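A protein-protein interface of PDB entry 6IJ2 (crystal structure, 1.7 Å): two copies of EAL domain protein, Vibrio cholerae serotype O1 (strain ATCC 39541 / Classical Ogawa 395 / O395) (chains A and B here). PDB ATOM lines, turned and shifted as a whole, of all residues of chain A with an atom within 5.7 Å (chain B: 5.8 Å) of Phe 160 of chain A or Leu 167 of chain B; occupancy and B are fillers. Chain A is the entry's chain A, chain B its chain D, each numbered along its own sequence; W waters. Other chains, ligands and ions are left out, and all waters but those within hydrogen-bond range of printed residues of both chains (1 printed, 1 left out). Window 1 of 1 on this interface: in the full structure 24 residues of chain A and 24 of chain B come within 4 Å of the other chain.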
ATOM      1  N   ILE A 157      27.829 -33.974  21.532  1.00  0.00           N
ATOM      2  CA  ILE A 157      27.606 -32.977  22.579  1.00  0.00           C
ATOM      3  C   ILE A 157      26.734 -33.623  23.651  1.00  0.00           C
ATOM      4  O   ILE A 157      25.640 -34.108  23.364  1.00  0.00           O
ATOM      5  CB  ILE A 157      26.954 -31.707  22.009  1.00  0.00           C
ATOM      6  CG1 ILE A 157      27.932 -31.025  21.048  1.00  0.00           C
ATOM      7  CG2 ILE A 157      26.546 -30.758  23.129  1.00  0.00           C
ATOM      8  CD1 ILE A 157      27.379 -29.813  20.390  1.00  0.00           C
ATOM      9  N   ASP A 158      27.238 -33.668  24.880  1.00  0.00           N
ATOM     10  CA  ASP A 158      26.597 -34.449  25.939  1.00  0.00           C
ATOM     11  C   ASP A 158      25.377 -33.740  26.530  1.00  0.00           C
ATOM     12  O   ASP A 158      24.344 -34.367  26.800  1.00  0.00           O
ATOM     13  CB  ASP A 158      27.643 -34.734  27.021  1.00  0.00           C
ATOM     14  CG  ASP A 158      27.246 -35.848  27.984  1.00  0.00           C
ATOM     15  OD1 ASP A 158      26.109 -36.355  27.940  1.00  0.00           O
ATOM     16  OD2 ASP A 158      28.118 -36.238  28.779  1.00  0.00           O
ATOM     17  N   ASP A 159      25.456 -32.442  26.743  1.00  0.00           N
ATOM     18  CA  ASP A 159      24.487 -31.854  27.648  1.00  0.00           C
ATOM     19  C   ASP A 159      23.755 -30.727  26.965  1.00  0.00           C
ATOM     20  O   ASP A 159      23.699 -29.616  27.477  1.00  0.00           O
ATOM     21  CB  ASP A 159      25.168 -31.357  28.928  1.00  0.00           C
ATOM     22  CG  ASP A 159      25.940 -32.460  29.669  1.00  0.00           C
ATOM     23  OD1 ASP A 159      25.717 -33.664  29.407  1.00  0.00           O
ATOM     24  OD2 ASP A 159      26.772 -32.110  30.539  1.00  0.00           O
ATOM     25  N   PHE A 160      23.177 -30.986  25.794  1.00  0.00           N
ATOM     26  CA  PHE A 160      22.393 -29.948  25.135  1.00  0.00           C
ATOM     27  C   PHE A 160      21.118 -29.658  25.918  1.00  0.00           C
ATOM     28  O   PHE A 160      20.316 -30.552  26.190  1.00  0.00           O
ATOM     29  CB  PHE A 160      22.033 -30.361  23.720  1.00  0.00           C
ATOM     30  CG  PHE A 160      21.387 -29.264  22.927  1.00  0.00           C
ATOM     31  CD1 PHE A 160      22.161 -28.375  22.206  1.00  0.00           C
ATOM     32  CD2 PHE A 160      20.016 -29.132  22.907  1.00  0.00           C
ATOM     33  CE1 PHE A 160      21.569 -27.378  21.461  1.00  0.00           C
ATOM     34  CE2 PHE A 160      19.409 -28.120  22.174  1.00  0.00           C
ATOM     35  CZ  PHE A 160      20.190 -27.252  21.452  1.00  0.00           C
ATOM     36  N   GLY A 161      20.906 -28.397  26.238  1.00  0.00           N
ATOM     37  CA  GLY A 161      19.732 -28.008  26.986  1.00  0.00           C
ATOM     38  C   GLY A 161      19.924 -27.904  28.478  1.00  0.00           C
ATOM     39  O   GLY A 161      18.937 -27.688  29.197  1.00  0.00           O
ATOM     40  N   SER A 162      21.156 -28.037  28.967  1.00  0.00           N
ATOM     41  CA  SER A 162      21.455 -27.764  30.367  1.00  0.00           C
ATOM     42  C   SER A 162      22.864 -27.202  30.469  1.00  0.00           C
ATOM     43  O   SER A 162      23.614 -27.183  29.499  1.00  0.00           O
ATOM     44  CB  SER A 162      21.333 -29.024  31.219  1.00  0.00           C
ATOM     45  OG  SER A 162      22.333 -29.949  30.841  1.00  0.00           O
ATOM     46  N   GLY A 166      24.691 -24.989  24.598  1.00  0.00           N
ATOM     47  CA  GLY A 166      24.982 -25.899  23.504  1.00  0.00           C
ATOM     48  C   GLY A 166      24.875 -25.240  22.147  1.00  0.00           C
ATOM     49  O   GLY A 166      25.579 -25.628  21.211  1.00  0.00           O
ATOM     50  N   LEU A 167      24.005 -24.228  22.010  1.00  0.00           N
ATOM     51  CA  LEU A 167      23.943 -23.522  20.734  1.00  0.00           C
ATOM     52  C   LEU A 167      25.239 -22.786  20.457  1.00  0.00           C
ATOM     53  O   LEU A 167      25.643 -22.660  19.296  1.00  0.00           O
ATOM     54  CB  LEU A 167      22.753 -22.554  20.699  1.00  0.00           C
ATOM     55  CG  LEU A 167      21.400 -23.264  20.566  1.00  0.00           C
ATOM     56  CD1 LEU A 167      20.258 -22.241  20.558  1.00  0.00           C
ATOM     57  CD2 LEU A 167      21.352 -24.161  19.312  1.00  0.00           C
ATOM     58  N   LEU A 170      27.326 -25.481  18.729  1.00  0.00           N
ATOM     59  CA  LEU A 170      26.837 -25.894  17.412  1.00  0.00           C
ATOM     60  C   LEU A 170      27.033 -24.829  16.346  1.00  0.00           C
ATOM     61  O   LEU A 170      27.061 -25.164  15.156  1.00  0.00           O
ATOM     62  CB  LEU A 170      25.352 -26.236  17.481  1.00  0.00           C
ATOM     63  CG  LEU A 170      25.014 -27.482  18.274  1.00  0.00           C
ATOM     64  CD1 LEU A 170      23.519 -27.704  18.262  1.00  0.00           C
ATOM     65  CD2 LEU A 170      25.735 -28.637  17.622  1.00  0.00           C
ATOM     66  N   VAL A 178      23.988 -35.186  19.028  1.00  0.00           N
ATOM     67  CA  VAL A 178      23.731 -34.245  20.120  1.00  0.00           C
ATOM     68  C   VAL A 178      22.802 -34.947  21.095  1.00  0.00           C
ATOM     69  O   VAL A 178      21.716 -35.397  20.705  1.00  0.00           O
ATOM     70  CB  VAL A 178      23.143 -32.913  19.627  1.00  0.00           C
ATOM     71  CG1 VAL A 178      22.626 -32.089  20.810  1.00  0.00           C
ATOM     72  CG2 VAL A 178      24.219 -32.093  18.973  1.00  0.00           C
ATOM     73  N   LYS A 179      23.257 -35.106  22.342  1.00  0.00           N
ATOM     74  CA  LYS A 179      22.446 -35.711  23.394  1.00  0.00           C
ATOM     75  C   LYS A 179      21.633 -34.623  24.073  1.00  0.00           C
ATOM     76  O   LYS A 179      22.190 -33.608  24.494  1.00  0.00           O
ATOM     77  CB  LYS A 179      23.324 -36.437  24.419  1.00  0.00           C
ATOM     78  CG  LYS A 179      24.105 -37.562  23.762  1.00  0.00           C
ATOM     79  CD  LYS A 179      23.939 -38.905  24.490  1.00  0.00           C
ATOM     80  CE  LYS A 179      24.793 -39.004  25.663  1.00  0.00           C
ATOM     81  NZ  LYS A 179      24.734 -40.347  26.353  1.00  0.00           N
ATOM     82  N   VAL A 180      20.323 -34.827  24.173  1.00  0.00           N
ATOM     83  CA  VAL A 180      19.429 -33.804  24.721  1.00  0.00           C
ATOM     84  C   VAL A 180      19.188 -34.111  26.187  1.00  0.00           C
ATOM     85  O   VAL A 180      18.700 -35.197  26.532  1.00  0.00           O
ATOM     86  CB  VAL A 180      18.108 -33.729  23.943  1.00  0.00           C
ATOM     87  CG1 VAL A 180      17.194 -32.663  24.581  1.00  0.00           C
ATOM     88  CG2 VAL A 180      18.385 -33.383  22.495  1.00  0.00           C
ATOM     89  N   ASP A 181      19.486 -33.124  27.038  1.00  0.00           N
ATOM     90  CA  ASP A 181      19.413 -33.299  28.480  1.00  0.00           C
ATOM     91  C   ASP A 181      18.011 -33.720  28.900  1.00  0.00           C
ATOM     92  O   ASP A 181      17.010 -33.274  28.333  1.00  0.00           O
ATOM     93  CB  ASP A 181      19.787 -31.989  29.177  1.00  0.00           C
ATOM     94  CG  ASP A 181      19.768 -32.108  30.679  1.00  0.00           C
ATOM     95  OD1 ASP A 181      20.705 -32.698  31.237  1.00  0.00           O
ATOM     96  OD2 ASP A 181      18.812 -31.624  31.307  1.00  0.00           O
ATOM     97  N   LEU A 184      14.929 -31.257  29.374  1.00  0.00           N
ATOM     98  CA  LEU A 184      14.097 -30.828  28.255  1.00  0.00           C
ATOM     99  C   LEU A 184      13.060 -31.858  27.847  1.00  0.00           C
ATOM    100  O   LEU A 184      12.060 -31.495  27.221  1.00  0.00           O
ATOM    101  CB  LEU A 184      14.948 -30.507  27.027  1.00  0.00           C
ATOM    102  CG  LEU A 184      15.827 -29.261  27.080  1.00  0.00           C
ATOM    103  CD1 LEU A 184      16.414 -29.025  25.681  1.00  0.00           C
ATOM    104  CD2 LEU A 184      15.047 -28.043  27.593  1.00  0.00           C
ATOM    105  N   ILE A 197      10.123 -26.474  22.031  1.00  0.00           N
ATOM    106  CA  ILE A 197      11.588 -26.480  22.051  1.00  0.00           C
ATOM    107  C   ILE A 197      12.120 -27.673  21.272  1.00  0.00           C
ATOM    108  O   ILE A 197      13.024 -27.544  20.437  1.00  0.00           O
ATOM    109  CB  ILE A 197      12.119 -26.481  23.498  1.00  0.00           C
ATOM    110  CG1 ILE A 197      11.811 -25.159  24.189  1.00  0.00           C
ATOM    111  CG2 ILE A 197      13.637 -26.709  23.515  1.00  0.00           C
ATOM    112  CD1 ILE A 197      12.282 -25.121  25.642  1.00  0.00           C
ATOM    113  N   CYS A 201      14.220 -27.648  17.818  1.00  0.00           N
ATOM    114  CA  CYS A 201      15.590 -28.148  17.889  1.00  0.00           C
ATOM    115  C   CYS A 201      15.810 -29.343  16.957  1.00  0.00           C
ATOM    116  O   CYS A 201      16.882 -29.473  16.364  1.00  0.00           O
ATOM    117  CB  CYS A 201      15.951 -28.540  19.318  1.00  0.00           C
ATOM    118  SG  CYS A 201      16.207 -27.106  20.391  1.00  0.00           S
ATOM    119  N   LEU A 204      16.432 -27.991  13.653  1.00  0.00           N
ATOM    120  CA  LEU A 204      17.794 -27.480  13.643  1.00  0.00           C
ATOM    121  C   LEU A 204      18.819 -28.612  13.503  1.00  0.00           C
ATOM    122  O   LEU A 204      19.763 -28.509  12.716  1.00  0.00           O
ATOM    123  CB  LEU A 204      18.045 -26.667  14.916  1.00  0.00           C
ATOM    124  CG  LEU A 204      19.506 -26.274  15.106  1.00  0.00           C
ATOM    125  CD1 LEU A 204      19.992 -25.522  13.883  1.00  0.00           C
ATOM    126  CD2 LEU A 204      19.636 -25.425  16.358  1.00  0.00           C
ATOM    127  N   PHE A 205      18.668 -29.687  14.275  1.00  0.00           N
ATOM    128  CA  PHE A 205      19.638 -30.788  14.200  1.00  0.00           C
ATOM    129  C   PHE A 205      19.694 -31.393  12.802  1.00  0.00           C
ATOM    130  O   PHE A 205      20.777 -31.694  12.287  1.00  0.00           O
ATOM    131  CB  PHE A 205      19.293 -31.872  15.214  1.00  0.00           C
ATOM    132  CG  PHE A 205      19.351 -31.412  16.640  1.00  0.00           C
ATOM    133  CD1 PHE A 205      20.221 -30.411  17.030  1.00  0.00           C
ATOM    134  CD2 PHE A 205      18.519 -31.981  17.590  1.00  0.00           C
ATOM    135  CE1 PHE A 205      20.273 -29.987  18.356  1.00  0.00           C
ATOM    136  CE2 PHE A 205      18.558 -31.570  18.910  1.00  0.00           C
ATOM    137  CZ  PHE A 205      19.434 -30.561  19.295  1.00  0.00           C
ATOM    138  N   PHE B 160      21.194 -15.225  25.189  1.00  0.00           N
ATOM    139  CA  PHE B 160      20.794 -16.462  24.525  1.00  0.00           C
ATOM    140  C   PHE B 160      21.808 -16.826  23.447  1.00  0.00           C
ATOM    141  O   PHE B 160      22.097 -16.022  22.557  1.00  0.00           O
ATOM    142  CB  PHE B 160      19.404 -16.307  23.920  1.00  0.00           C
ATOM    143  CG  PHE B 160      18.857 -17.588  23.360  1.00  0.00           C
ATOM    144  CD1 PHE B 160      19.098 -17.933  22.040  1.00  0.00           C
ATOM    145  CD2 PHE B 160      18.142 -18.460  24.167  1.00  0.00           C
ATOM    146  CE1 PHE B 160      18.613 -19.108  21.517  1.00  0.00           C
ATOM    147  CE2 PHE B 160      17.658 -19.655  23.643  1.00  0.00           C
ATOM    148  CZ  PHE B 160      17.891 -19.968  22.323  1.00  0.00           C
ATOM    149  N   SER B 165      23.139 -22.206  29.364  1.00  0.00           N
ATOM    150  CA  SER B 165      22.113 -22.669  28.421  1.00  0.00           C
ATOM    151  C   SER B 165      20.843 -21.829  28.538  1.00  0.00           C
ATOM    152  O   SER B 165      20.149 -21.875  29.556  1.00  0.00           O
ATOM    153  CB  SER B 165      21.806 -24.146  28.667  1.00  0.00           C
ATOM    154  OG  SER B 165      20.666 -24.577  27.924  1.00  0.00           O
ATOM    155  N   GLY B 166      20.519 -21.090  27.470  1.00  0.00           N
ATOM    156  CA  GLY B 166      19.274 -20.345  27.431  1.00  0.00           C
ATOM    157  C   GLY B 166      18.051 -21.232  27.320  1.00  0.00           C
ATOM    158  O   GLY B 166      16.989 -20.902  27.862  1.00  0.00           O
ATOM    159  N   LEU B 167      18.166 -22.366  26.608  1.00  0.00           N
ATOM    160  CA  LEU B 167      17.012 -23.252  26.496  1.00  0.00           C
ATOM    161  C   LEU B 167      16.635 -23.841  27.840  1.00  0.00           C
ATOM    162  O   LEU B 167      15.455 -24.114  28.089  1.00  0.00           O
ATOM    163  CB  LEU B 167      17.295 -24.387  25.500  1.00  0.00           C
ATOM    164  CG  LEU B 167      17.465 -23.913  24.059  1.00  0.00           C
ATOM    165  CD1 LEU B 167      17.998 -25.064  23.196  1.00  0.00           C
ATOM    166  CD2 LEU B 167      16.144 -23.381  23.519  1.00  0.00           C
ATOM    167  N   ASN B 168      17.626 -24.081  28.704  1.00  0.00           N
ATOM    168  CA  ASN B 168      17.339 -24.534  30.057  1.00  0.00           C
ATOM    169  C   ASN B 168      16.420 -23.547  30.771  1.00  0.00           C
ATOM    170  O   ASN B 168      15.540 -23.945  31.549  1.00  0.00           O
ATOM    171  CB  ASN B 168      18.651 -24.709  30.822  1.00  0.00           C
ATOM    172  CG  ASN B 168      18.451 -25.236  32.219  1.00  0.00           C
ATOM    173  OD1 ASN B 168      17.678 -26.167  32.443  1.00  0.00           O
ATOM    174  ND2 ASN B 168      19.150 -24.637  33.176  1.00  0.00           N
ATOM    175  N   LEU B 169      16.621 -22.260  30.519  1.00  0.00           N
ATOM    176  CA  LEU B 169      15.759 -21.244  31.110  1.00  0.00           C
ATOM    177  C   LEU B 169      14.386 -21.262  30.454  1.00  0.00           C
ATOM    178  O   LEU B 169      13.366 -21.395  31.142  1.00  0.00           O
ATOM    179  CB  LEU B 169      16.403 -19.865  30.967  1.00  0.00           C
ATOM    180  CG  LEU B 169      17.786 -19.689  31.596  1.00  0.00           C
ATOM    181  CD1 LEU B 169      18.243 -18.235  31.456  1.00  0.00           C
ATOM    182  CD2 LEU B 169      17.746 -20.102  33.051  1.00  0.00           C
ATOM    183  N   LEU B 170      14.356 -21.193  29.115  1.00  0.00           N
ATOM    184  CA  LEU B 170      13.095 -21.038  28.392  1.00  0.00           C
ATOM    185  C   LEU B 170      12.162 -22.220  28.609  1.00  0.00           C
ATOM    186  O   LEU B 170      10.943 -22.074  28.475  1.00  0.00           O
ATOM    187  CB  LEU B 170      13.355 -20.859  26.898  1.00  0.00           C
ATOM    188  CG  LEU B 170      13.937 -19.519  26.488  1.00  0.00           C
ATOM    189  CD1 LEU B 170      14.174 -19.462  24.991  1.00  0.00           C
ATOM    190  CD2 LEU B 170      12.980 -18.435  26.940  1.00  0.00           C
ATOM    191  N   ALA B 171      12.716 -23.400  28.915  1.00  0.00           N
ATOM    192  CA  ALA B 171      11.887 -24.571  29.149  1.00  0.00           C
ATOM    193  C   ALA B 171      10.942 -24.393  30.333  1.00  0.00           C
ATOM    194  O   ALA B 171       9.903 -25.063  30.400  1.00  0.00           O
ATOM    195  CB  ALA B 171      12.780 -25.808  29.366  1.00  0.00           C
ATOM    196  N   ASP B 172      11.275 -23.518  31.283  1.00  0.00           N
ATOM    197  CA  ASP B 172      10.497 -23.421  32.506  1.00  0.00           C
ATOM    198  C   ASP B 172       9.902 -22.040  32.770  1.00  0.00           C
ATOM    199  O   ASP B 172       9.038 -21.924  33.646  1.00  0.00           O
ATOM    200  CB  ASP B 172      11.346 -23.855  33.710  1.00  0.00           C
ATOM    201  CG  ASP B 172      11.464 -25.370  33.825  1.00  0.00           C
ATOM    202  OD1 ASP B 172      10.415 -26.053  33.869  1.00  0.00           O
ATOM    203  OD2 ASP B 172      12.602 -25.877  33.875  1.00  0.00           O
ATOM    204  N   LEU B 204      10.893 -20.963  17.201  1.00  0.00           N
ATOM    205  CA  LEU B 204      10.703 -21.263  18.621  1.00  0.00           C
ATOM    206  C   LEU B 204      10.164 -20.052  19.380  1.00  0.00           C
ATOM    207  O   LEU B 204       9.175 -20.152  20.120  1.00  0.00           O
ATOM    208  CB  LEU B 204      12.029 -21.717  19.233  1.00  0.00           C
ATOM    209  CG  LEU B 204      12.088 -22.596  20.486  1.00  0.00           C
ATOM    210  CD1 LEU B 204      13.239 -22.184  21.407  1.00  0.00           C
ATOM    211  CD2 LEU B 204      10.782 -22.699  21.239  1.00  0.00           C
HETATM  212  O   HOH W   1      21.951 -25.589  25.487  1.00  0.00           O
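N of Phe 160 of chain A sits at hydrogen-bond distance from O of Lys 179 of chain A (3.1 Å).
The backbone carbonyl oxygen (O) of Phe 160 of chain A lies within hydrogen-bond range of the backbone NH (N) of Asp 181 of chain A.
The side-chain hydroxyl (OG) of Ser 162 of chain A is in hydrogen-bond range of the side-chain carboxylate (OD1) of Asp 181 of chain A.
O of Ile 197 of chain A lies within hydrogen-bond range of SG of Cys 201 of chain A, at 3.2 Å.
N of Asn 168 of chain B sits at hydrogen-bond distance from OG of Ser 165 of chain B (3.2 Å).
Printed residues of chain A that touch a printed residue of chain B: Phe 160, Gly 161, Ser 162, Leu 167, Leu 184, Ile 197 and Cys 201.
Hydrophobic or aromatic side chains of chain A within 4 Å of the printed part of chain B: Phe 160, Leu 167, Leu 184 and Ile 197.
Water W1 lies within hydrogen-bond range of OG of Ser 165 of chain B, N of Gly 166 of chain A and N of Gly 161 of chain A.
Of chain B, only Leu 167 comes within 4 Å of Phe 160 of chain A.
Of the printed residues of chain A, Leu 167 of chain B touches Phe 160, Leu 184 and Cys 201.
Printed residues of chain A within 4 Å of Leu 204 of chain B: Ile 197.
Printed residues of chain B within 4 Å of Leu 184 of chain A: Leu 167 (3.98 Å) and Ala 171 (3.6 Å).
Of the printed residues of chain B, Gly 161 of chain A touches Ser 165 (3.5 Å) and Asn 168 (3.4 Å).
Printed residues of chain B within 4 Å of Ile 197 of chain A: Ala 171 and Leu 204.
Leu 170 of chain A touches none of the printed residues of chain B.
The nearest printed residue of chain B that does not touch Ile 197 of chain A is Leu 167 of chain B (4.1 Å).
CD1 of Leu 167 of chain B touches CE2 of Phe 160 of chain A (3.5 Å).
Gly 161 of chain A touches Ser 165 of chain B.
O of Gly 161 of chain A touches CB of Asn 168 of chain B, at 3.4 Å.
Ser 165 of chain B touches Ser 162 of chain A (CB to O, 3.6 Å).
Leu 167 of chain A touches Phe 160 of chain B.
CD2 of Leu 184 of chain A touches O of Leu 167 of chain B, at 3.98 Å.
Leu 184 of chain A touches Ala 171 of chain B.
Ala 171 of chain B touches Ile 197 of chain A (CA to CD1, 3.6 Å).
Ile 197 of chain A touches Leu 204 of chain B.
CD1 of Leu 167 of chain B touches SG of Cys 201 of chain A, 3.9 Å away.
Phe 160 of chain A touches Leu 167 of chain B, and with the chains exchanged Leu 167 of chain A touches Phe 160 of chain B.
Positions printed for both chains: 160, 166, 167, 170 and 204.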
